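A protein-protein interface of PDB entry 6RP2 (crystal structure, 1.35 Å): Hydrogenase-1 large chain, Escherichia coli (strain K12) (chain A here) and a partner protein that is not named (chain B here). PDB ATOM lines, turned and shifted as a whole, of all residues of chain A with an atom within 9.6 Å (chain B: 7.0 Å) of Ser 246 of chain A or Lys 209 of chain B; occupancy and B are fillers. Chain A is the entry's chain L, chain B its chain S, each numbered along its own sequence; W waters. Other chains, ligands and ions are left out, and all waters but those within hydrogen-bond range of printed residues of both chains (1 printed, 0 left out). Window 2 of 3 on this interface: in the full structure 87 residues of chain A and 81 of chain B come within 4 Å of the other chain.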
ATOM      1  N   PRO A 238     -38.829   4.146 -25.301  1.00  0.00           N
ATOM      2  CA  PRO A 238     -37.518   4.087 -24.669  1.00  0.00           C
ATOM      3  C   PRO A 238     -36.459   3.330 -25.463  1.00  0.00           C
ATOM      4  O   PRO A 238     -35.331   3.316 -25.028  1.00  0.00           O
ATOM      5  CB  PRO A 238     -37.794   3.415 -23.327  1.00  0.00           C
ATOM      6  CG  PRO A 238     -39.058   2.684 -23.462  1.00  0.00           C
ATOM      7  CD  PRO A 238     -39.775   3.222 -24.674  1.00  0.00           C
ATOM      8  N   CYS A 239     -36.843   2.730 -26.589  1.00  0.00           N
ATOM      9  CA  CYS A 239     -35.963   1.893 -27.407  1.00  0.00           C
ATOM     10  C   CYS A 239     -35.108   2.771 -28.309  1.00  0.00           C
ATOM     11  O   CYS A 239     -35.310   2.812 -29.540  1.00  0.00           O
ATOM     12  CB  CYS A 239     -36.783   0.853 -28.149  1.00  0.00           C
ATOM     13  SG  CYS A 239     -38.171   1.535 -29.102  1.00  0.00           S
ATOM     14  N   ALA A 240     -34.145   3.445 -27.704  1.00  0.00           N
ATOM     15  CA  ALA A 240     -33.173   4.287 -28.407  1.00  0.00           C
ATOM     16  C   ALA A 240     -32.543   3.499 -29.553  1.00  0.00           C
ATOM     17  O   ALA A 240     -32.283   2.278 -29.413  1.00  0.00           O
ATOM     18  CB  ALA A 240     -32.122   4.796 -27.447  1.00  0.00           C
ATOM     19  N   ILE A 241     -32.299   4.210 -30.648  1.00  0.00           N
ATOM     20  CA  ILE A 241     -31.753   3.650 -31.898  1.00  0.00           C
ATOM     21  C   ILE A 241     -30.295   4.046 -32.031  1.00  0.00           C
ATOM     22  O   ILE A 241     -29.917   5.219 -31.816  1.00  0.00           O
ATOM     23  CB  ILE A 241     -32.591   4.070 -33.096  1.00  0.00           C
ATOM     24  CG1 ILE A 241     -34.037   3.599 -32.947  1.00  0.00           C
ATOM     25  CG2 ILE A 241     -31.963   3.588 -34.409  1.00  0.00           C
ATOM     26  CD1 ILE A 241     -34.986   4.146 -33.940  1.00  0.00           C
ATOM     27  N   ASN A 242     -29.476   3.105 -32.462  1.00  0.00           N
ATOM     28  CA  ASN A 242     -28.056   3.375 -32.819  1.00  0.00           C
ATOM     29  C   ASN A 242     -27.699   2.364 -33.893  1.00  0.00           C
ATOM     30  O   ASN A 242     -27.681   1.140 -33.581  1.00  0.00           O
ATOM     31  CB  ASN A 242     -27.158   3.254 -31.594  1.00  0.00           C
ATOM     32  CG  ASN A 242     -25.690   3.481 -31.882  1.00  0.00           C
ATOM     33  OD1 ASN A 242     -25.280   3.543 -33.045  1.00  0.00           O
ATOM     34  ND2 ASN A 242     -24.915   3.571 -30.829  1.00  0.00           N
ATOM     35  N   ILE A 243     -27.486   2.816 -35.133  1.00  0.00           N
ATOM     36  CA  ILE A 243     -27.195   1.935 -36.303  1.00  0.00           C
ATOM     37  C   ILE A 243     -25.689   1.861 -36.538  1.00  0.00           C
ATOM     38  O   ILE A 243     -25.193   0.787 -36.817  1.00  0.00           O
ATOM     39  CB  ILE A 243     -27.886   2.446 -37.586  1.00  0.00           C
ATOM     40  CG1 ILE A 243     -29.373   2.683 -37.346  1.00  0.00           C
ATOM     41  CG2 ILE A 243     -27.652   1.456 -38.718  1.00  0.00           C
ATOM     42  CD1 ILE A 243     -30.066   1.409 -36.775  1.00  0.00           C
ATOM     43  N   ASP A 244     -24.974   2.963 -36.441  1.00  0.00           N
ATOM     44  CA  ASP A 244     -23.609   3.038 -37.044  1.00  0.00           C
ATOM     45  C   ASP A 244     -22.603   3.690 -36.104  1.00  0.00           C
ATOM     46  O   ASP A 244     -21.542   4.130 -36.568  1.00  0.00           O
ATOM     47  CB  ASP A 244     -23.651   3.786 -38.378  1.00  0.00           C
ATOM     48  CG  ASP A 244     -22.393   3.676 -39.232  1.00  0.00           C
ATOM     49  OD1 ASP A 244     -21.797   2.573 -39.276  1.00  0.00           O
ATOM     50  OD2 ASP A 244     -22.029   4.700 -39.837  1.00  0.00           O
ATOM     51  N   GLU A 245     -22.874   3.730 -34.809  1.00  0.00           N
ATOM     52  CA  GLU A 245     -21.994   4.345 -33.812  1.00  0.00           C
ATOM     53  C   GLU A 245     -21.564   3.320 -32.782  1.00  0.00           C
ATOM     54  O   GLU A 245     -22.200   2.223 -32.640  1.00  0.00           O
ATOM     55  CB  GLU A 245     -22.688   5.533 -33.138  1.00  0.00           C
ATOM     56  CG  GLU A 245     -23.037   6.635 -34.132  1.00  0.00           C
ATOM     57  CD  GLU A 245     -24.051   7.583 -33.525  1.00  0.00           C
ATOM     58  OE1 GLU A 245     -23.590   8.307 -32.652  1.00  0.00           O
ATOM     59  OE2 GLU A 245     -25.309   7.456 -33.832  1.00  0.00           O
ATOM     60  N   SER A 246     -20.488   3.636 -32.084  1.00  0.00           N
ATOM     61  CA  SER A 246     -20.022   2.811 -30.961  1.00  0.00           C
ATOM     62  C   SER A 246     -21.180   2.554 -30.000  1.00  0.00           C
ATOM     63  O   SER A 246     -21.968   3.498 -29.731  1.00  0.00           O
ATOM     64  CB  SER A 246     -18.854   3.444 -30.272  1.00  0.00           C
ATOM     65  OG  SER A 246     -18.372   2.579 -29.287  1.00  0.00           O
ATOM     66  N   GLY A 247     -21.269   1.336 -29.488  1.00  0.00           N
ATOM     67  CA  GLY A 247     -22.309   1.048 -28.512  1.00  0.00           C
ATOM     68  C   GLY A 247     -23.649   0.695 -29.145  1.00  0.00           C
ATOM     69  O   GLY A 247     -24.648   0.562 -28.390  1.00  0.00           O
ATOM     70  N   ALA A 248     -23.728   0.469 -30.456  1.00  0.00           N
ATOM     71  CA  ALA A 248     -24.997   0.044 -31.084  1.00  0.00           C
ATOM     72  C   ALA A 248     -25.445  -1.272 -30.480  1.00  0.00           C
ATOM     73  O   ALA A 248     -26.669  -1.560 -30.524  1.00  0.00           O
ATOM     74  CB  ALA A 248     -24.871  -0.047 -32.570  1.00  0.00           C
ATOM     75  N   VAL A 249     -24.543  -2.061 -29.903  1.00  0.00           N
ATOM     76  CA  VAL A 249     -24.891  -3.309 -29.158  1.00  0.00           C
ATOM     77  C   VAL A 249     -25.868  -3.011 -28.025  1.00  0.00           C
ATOM     78  O   VAL A 249     -26.506  -3.970 -27.539  1.00  0.00           O
ATOM     79  CB  VAL A 249     -23.641  -4.025 -28.638  1.00  0.00           C
ATOM     80  CG1 VAL A 249     -22.835  -4.612 -29.805  1.00  0.00           C
ATOM     81  CG2 VAL A 249     -22.797  -3.162 -27.755  1.00  0.00           C
ATOM     82  N   GLY A 250     -25.903  -1.774 -27.548  1.00  0.00           N
ATOM     83  CA  GLY A 250     -26.779  -1.390 -26.436  1.00  0.00           C
ATOM     84  C   GLY A 250     -28.073  -0.766 -26.899  1.00  0.00           C
ATOM     85  O   GLY A 250     -28.753  -0.130 -26.041  1.00  0.00           O
ATOM     86  N   ALA A 251     -28.478  -0.874 -28.166  1.00  0.00           N
ATOM     87  CA  ALA A 251     -29.609  -0.106 -28.705  1.00  0.00           C
ATOM     88  C   ALA A 251     -30.302  -0.871 -29.817  1.00  0.00           C
ATOM     89  O   ALA A 251     -29.879  -2.002 -30.143  1.00  0.00           O
ATOM     90  CB  ALA A 251     -29.109   1.228 -29.213  1.00  0.00           C
ATOM     91  N   VAL A 252     -31.335  -0.288 -30.394  1.00  0.00           N
ATOM     92  CA  VAL A 252     -31.974  -0.871 -31.586  1.00  0.00           C
ATOM     93  C   VAL A 252     -31.042  -0.610 -32.763  1.00  0.00           C
ATOM     94  O   VAL A 252     -30.828   0.514 -33.154  1.00  0.00           O
ATOM     95  CB  VAL A 252     -33.353  -0.275 -31.827  1.00  0.00           C
ATOM     96  CG1 VAL A 252     -33.932  -0.747 -33.144  1.00  0.00           C
ATOM     97  CG2 VAL A 252     -34.311  -0.593 -30.707  1.00  0.00           C
ATOM     98  N   ASN A 253     -30.423  -1.676 -33.244  1.00  0.00           N
ATOM     99  CA  ASN A 253     -29.355  -1.640 -34.255  1.00  0.00           C
ATOM    100  C   ASN A 253     -29.845  -2.422 -35.478  1.00  0.00           C
ATOM    101  O   ASN A 253     -30.965  -2.891 -35.515  1.00  0.00           O
ATOM    102  CB  ASN A 253     -28.060  -2.163 -33.621  1.00  0.00           C
ATOM    103  CG  ASN A 253     -28.161  -3.599 -33.173  1.00  0.00           C
ATOM    104  OD1 ASN A 253     -28.717  -4.425 -33.867  1.00  0.00           O
ATOM    105  ND2 ASN A 253     -27.644  -3.915 -31.992  1.00  0.00           N
ATOM    106  N   ARG B 189     -25.986  -4.557 -18.216  1.00  0.00           N
ATOM    107  CA  ARG B 189     -25.578  -3.137 -18.101  1.00  0.00           C
ATOM    108  C   ARG B 189     -24.896  -2.873 -16.764  1.00  0.00           C
ATOM    109  O   ARG B 189     -24.574  -1.685 -16.502  1.00  0.00           O
ATOM    110  CB  ARG B 189     -26.772  -2.209 -18.324  1.00  0.00           C
ATOM    111  CG  ARG B 189     -27.400  -2.329 -19.703  1.00  0.00           C
ATOM    112  CD  ARG B 189     -28.497  -1.336 -19.972  1.00  0.00           C
ATOM    113  NE  ARG B 189     -29.099  -1.568 -21.265  1.00  0.00           N
ATOM    114  CZ  ARG B 189     -29.736  -0.686 -22.009  1.00  0.00           C
ATOM    115  NH1 ARG B 189     -29.855   0.579 -21.613  1.00  0.00           N
ATOM    116  NH2 ARG B 189     -30.250  -1.036 -23.177  1.00  0.00           N
ATOM    117  N   HIS B 192     -21.878  -0.549 -16.630  1.00  0.00           N
ATOM    118  CA  HIS B 192     -22.153   0.903 -16.677  1.00  0.00           C
ATOM    119  C   HIS B 192     -22.545   1.392 -15.292  1.00  0.00           C
ATOM    120  O   HIS B 192     -22.074   2.460 -14.853  1.00  0.00           O
ATOM    121  CB  HIS B 192     -23.209   1.177 -17.730  1.00  0.00           C
ATOM    122  CG  HIS B 192     -22.804   0.772 -19.109  1.00  0.00           C
ATOM    123  ND1 HIS B 192     -21.631   1.231 -19.683  1.00  0.00           N
ATOM    124  CD2 HIS B 192     -23.392  -0.073 -19.988  1.00  0.00           C
ATOM    125  CE1 HIS B 192     -21.556   0.684 -20.910  1.00  0.00           C
ATOM    126  NE2 HIS B 192     -22.638  -0.122 -21.125  1.00  0.00           N
ATOM    127  N   VAL B 199     -27.990   6.638 -18.189  1.00  0.00           N
ATOM    128  CA  VAL B 199     -28.952   7.443 -18.950  1.00  0.00           C
ATOM    129  C   VAL B 199     -29.473   8.509 -17.977  1.00  0.00           C
ATOM    130  O   VAL B 199     -29.832   8.169 -16.839  1.00  0.00           O
ATOM    131  CB  VAL B 199     -30.095   6.549 -19.458  1.00  0.00           C
ATOM    132  CG1 VAL B 199     -31.169   7.330 -20.187  1.00  0.00           C
ATOM    133  CG2 VAL B 199     -29.535   5.448 -20.348  1.00  0.00           C
ATOM    134  N   ASP B 204     -30.851  10.157 -24.804  1.00  0.00           N
ATOM    135  CA  ASP B 204     -29.565  10.883 -24.712  1.00  0.00           C
ATOM    136  C   ASP B 204     -28.446   9.969 -25.247  1.00  0.00           C
ATOM    137  O   ASP B 204     -28.672   8.819 -25.676  1.00  0.00           O
ATOM    138  CB  ASP B 204     -29.340  11.424 -23.300  1.00  0.00           C
ATOM    139  CG  ASP B 204     -29.124  10.420 -22.194  1.00  0.00           C
ATOM    140  OD1 ASP B 204     -29.090   9.203 -22.497  1.00  0.00           O
ATOM    141  OD2 ASP B 204     -28.962  10.834 -21.005  1.00  0.00           O
ATOM    142  N   ASP B 205     -27.226  10.483 -25.282  1.00  0.00           N
ATOM    143  CA  ASP B 205     -26.117   9.720 -25.883  1.00  0.00           C
ATOM    144  C   ASP B 205     -25.899   8.446 -25.084  1.00  0.00           C
ATOM    145  O   ASP B 205     -25.616   7.376 -25.682  1.00  0.00           O
ATOM    146  CB  ASP B 205     -24.892  10.628 -25.990  1.00  0.00           C
ATOM    147  CG  ASP B 205     -25.038  11.699 -27.071  1.00  0.00           C
ATOM    148  OD1 ASP B 205     -25.992  11.670 -27.878  1.00  0.00           O
ATOM    149  OD2 ASP B 205     -24.123  12.522 -27.130  1.00  0.00           O
ATOM    150  N   ALA B 206     -26.046   8.518 -23.779  1.00  0.00           N
ATOM    151  CA  ALA B 206     -25.937   7.350 -22.887  1.00  0.00           C
ATOM    152  C   ALA B 206     -26.975   6.273 -23.255  1.00  0.00           C
ATOM    153  O   ALA B 206     -26.632   5.065 -23.332  1.00  0.00           O
ATOM    154  CB  ALA B 206     -26.084   7.782 -21.450  1.00  0.00           C
ATOM    155  N   ALA B 207     -28.205   6.691 -23.524  1.00  0.00           N
ATOM    156  CA  ALA B 207     -29.268   5.727 -23.874  1.00  0.00           C
ATOM    157  C   ALA B 207     -28.883   5.007 -25.149  1.00  0.00           C
ATOM    158  O   ALA B 207     -29.160   3.811 -25.297  1.00  0.00           O
ATOM    159  CB  ALA B 207     -30.569   6.444 -24.015  1.00  0.00           C
ATOM    160  N   ARG B 208     -28.326   5.725 -26.101  1.00  0.00           N
ATOM    161  CA  ARG B 208     -27.982   5.182 -27.433  1.00  0.00           C
ATOM    162  C   ARG B 208     -26.764   4.271 -27.364  1.00  0.00           C
ATOM    163  O   ARG B 208     -26.538   3.556 -28.370  1.00  0.00           O
ATOM    164  CB  ARG B 208     -27.791   6.305 -28.438  1.00  0.00           C
ATOM    165  CG  ARG B 208     -29.073   7.052 -28.759  1.00  0.00           C
ATOM    166  CD  ARG B 208     -28.805   8.236 -29.650  1.00  0.00           C
ATOM    167  NE  ARG B 208     -30.063   8.946 -29.901  1.00  0.00           N
ATOM    168  CZ  ARG B 208     -30.286   9.768 -30.924  1.00  0.00           C
ATOM    169  NH1 ARG B 208     -29.306  10.121 -31.750  1.00  0.00           N
ATOM    170  NH2 ARG B 208     -31.484  10.287 -31.059  1.00  0.00           N
ATOM    171  N   LYS B 209     -26.072   4.206 -26.236  1.00  0.00           N
ATOM    172  CA  LYS B 209     -24.935   3.273 -26.037  1.00  0.00           C
ATOM    173  C   LYS B 209     -25.320   2.162 -25.046  1.00  0.00           C
ATOM    174  O   LYS B 209     -24.454   1.370 -24.671  1.00  0.00           O
ATOM    175  CB  LYS B 209     -23.747   4.066 -25.473  1.00  0.00           C
ATOM    176  CG  LYS B 209     -23.067   5.044 -26.397  1.00  0.00           C
ATOM    177  CD  LYS B 209     -21.900   5.693 -25.686  1.00  0.00           C
ATOM    178  CE  LYS B 209     -22.278   6.775 -24.719  1.00  0.00           C
ATOM    179  NZ  LYS B 209     -21.064   7.573 -24.393  1.00  0.00           N
ATOM    180  N   GLY B 210     -26.568   2.145 -24.572  1.00  0.00           N
ATOM    181  CA  GLY B 210     -26.985   1.073 -23.648  1.00  0.00           C
ATOM    182  C   GLY B 210     -26.492   1.249 -22.228  1.00  0.00           C
ATOM    183  O   GLY B 210     -26.266   0.270 -21.556  1.00  0.00           O
ATOM    184  N   TYR B 211     -26.344   2.499 -21.750  1.00  0.00           N
ATOM    185  CA  TYR B 211     -25.906   2.733 -20.367  1.00  0.00           C
ATOM    186  C   TYR B 211     -27.013   2.343 -19.387  1.00  0.00           C
ATOM    187  O   TYR B 211     -28.172   2.032 -19.732  1.00  0.00           O
ATOM    188  CB  TYR B 211     -25.467   4.199 -20.222  1.00  0.00           C
ATOM    189  CG  TYR B 211     -24.089   4.522 -20.767  1.00  0.00           C
ATOM    190  CD1 TYR B 211     -23.357   3.627 -21.510  1.00  0.00           C
ATOM    191  CD2 TYR B 211     -23.521   5.759 -20.485  1.00  0.00           C
ATOM    192  CE1 TYR B 211     -22.087   3.938 -21.999  1.00  0.00           C
ATOM    193  CE2 TYR B 211     -22.249   6.064 -20.933  1.00  0.00           C
ATOM    194  CZ  TYR B 211     -21.568   5.180 -21.729  1.00  0.00           C
ATOM    195  OH  TYR B 211     -20.309   5.511 -22.194  1.00  0.00           O
ATOM    196  N   CYS B 212     -26.629   2.277 -18.117  1.00  0.00           N
ATOM    197  CA  CYS B 212     -27.458   1.793 -17.010  1.00  0.00           C
ATOM    198  C   CYS B 212     -28.659   2.734 -16.817  1.00  0.00           C
ATOM    199  O   CYS B 212     -28.523   3.950 -16.988  1.00  0.00           O
ATOM    200  CB  CYS B 212     -26.609   1.635 -15.762  1.00  0.00           C
ATOM    201  SG  CYS B 212     -27.572   1.355 -14.244  1.00  0.00           S
HETATM  202  O   HOH W   1     -31.276   0.671 -25.296  1.00  0.00           O
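The guanidinium group (NH2) of Arg 189 of chain B sits at hydrogen-bond distance from the backbone carbonyl oxygen (O) of Gly 250 of chain A (3.4 Å).
The side-chain amide nitrogen of Asn 242 of chain A sits at hydrogen-bond distance from the backbone carbonyl oxygen of Arg 208 of chain B (2.9 Å).
N of Gly 210 of chain B sits close to O of Gly 250 of chain A.
The backbone carbonyl oxygen (O) of Gly 210 of chain B lies close to the guanidinium group (NE) of Arg 189 of chain B, at 3.4 Å.
N of Ala 207 of chain B lies within hydrogen-bond range of OD1 of Asp 204 of chain B, at 2.9 Å.
OH of Tyr 211 of chain B lies within hydrogen-bond range of NZ of Lys 209 of chain B, 3.1 Å away.
O of Ala 240 of chain A lies within hydrogen-bond range of N of Val 252 of chain A.
The backbone carbonyl oxygen of Val 252 of chain A lies within hydrogen-bond range of the backbone NH of Asn 242 of chain A, at 3.0 Å.
The backbone carbonyl oxygen of Ala 251 of chain A is in hydrogen-bond range of the side-chain amide nitrogen of Asn 253 of chain A.
Among the printed residues, merely in contact across the chains: Ala 240 of chain A with Ala 207 of chain B (3.8 Å), Ile 241 of chain A with Arg 208 of chain B (3.7 Å), Ser 246 of chain A with Lys 209 of chain B (3.8 Å), Gly 247 of chain A with Arg 208 of chain B (3.5 Å), Gly 247 of chain A with Lys 209 of chain B (3.6 Å) and Ala 251 of chain A with Arg 208 of chain B (3.6 Å).
Ser 246 of chain A touches just one residue of chain B: Lys 209.
Of the printed residues of chain A, Lys 209 of chain B touches Ser 246 (3.8 Å) and Gly 247 (3.6 Å).
Ala 206 of chain B touches none of the printed residues of chain A.
Gly 210 of chain B touches just one residue of chain A: Gly 250.
Of the printed residues of chain B, Gly 247 of chain A touches Arg 208 and Lys 209.
Printed residues of chain B within 4 Å of Ala 251 of chain A: Arg 208.
Of the printed residues of chain A, Arg 208 of chain B touches Ile 241 (3.7 Å), Asn 242 (2.9 Å), Gly 247 (3.5 Å) and Ala 251 (3.6 Å).
Of the printed residues of chain B, Ile 241 of chain A touches Arg 208.
Of the printed residues of chain B, Asn 242 of chain A touches Arg 208.
Pro 238 of chain A touches none of the printed residues of chain B.
Cys 239 of chain A touches none of the printed residues of chain B.
The nearest residue of chain B that does not touch Ser 246 of chain A is Arg 208 of chain B (4.8 Å).
The nearest printed residue of chain A that does not touch Lys 209 of chain B is Gly 250 of chain A (4.02 Å).
Of the 12 printed residues of chain B, 5 touch a printed residue of chain A.
Of the 16 printed residues of chain A, 7 touch a printed residue of chain B.
Printed residues of chain A that touch a printed residue of chain B: Ala 240, Ile 241, Asn 242, Ser 246, Gly 247, Gly 250 and Ala 251.
Hydrophobic or aromatic side chains of chain A that line the printed part of chain B: Ala 240 and Ala 251.
Among the printed residues, 9 pairs touch across the chains.
Among the printed residues, no Asp or Glu carboxylate lies within 4 Å of a Lys or Arg side-chain nitrogen of the other chain.
Water W1 lies within hydrogen-bond range of the backbone carbonyl oxygen (O) of Gly 250 of chain A (2.7 Å) and the guanidinium group (NH2) of Arg 189 of chain B (2.9 Å).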
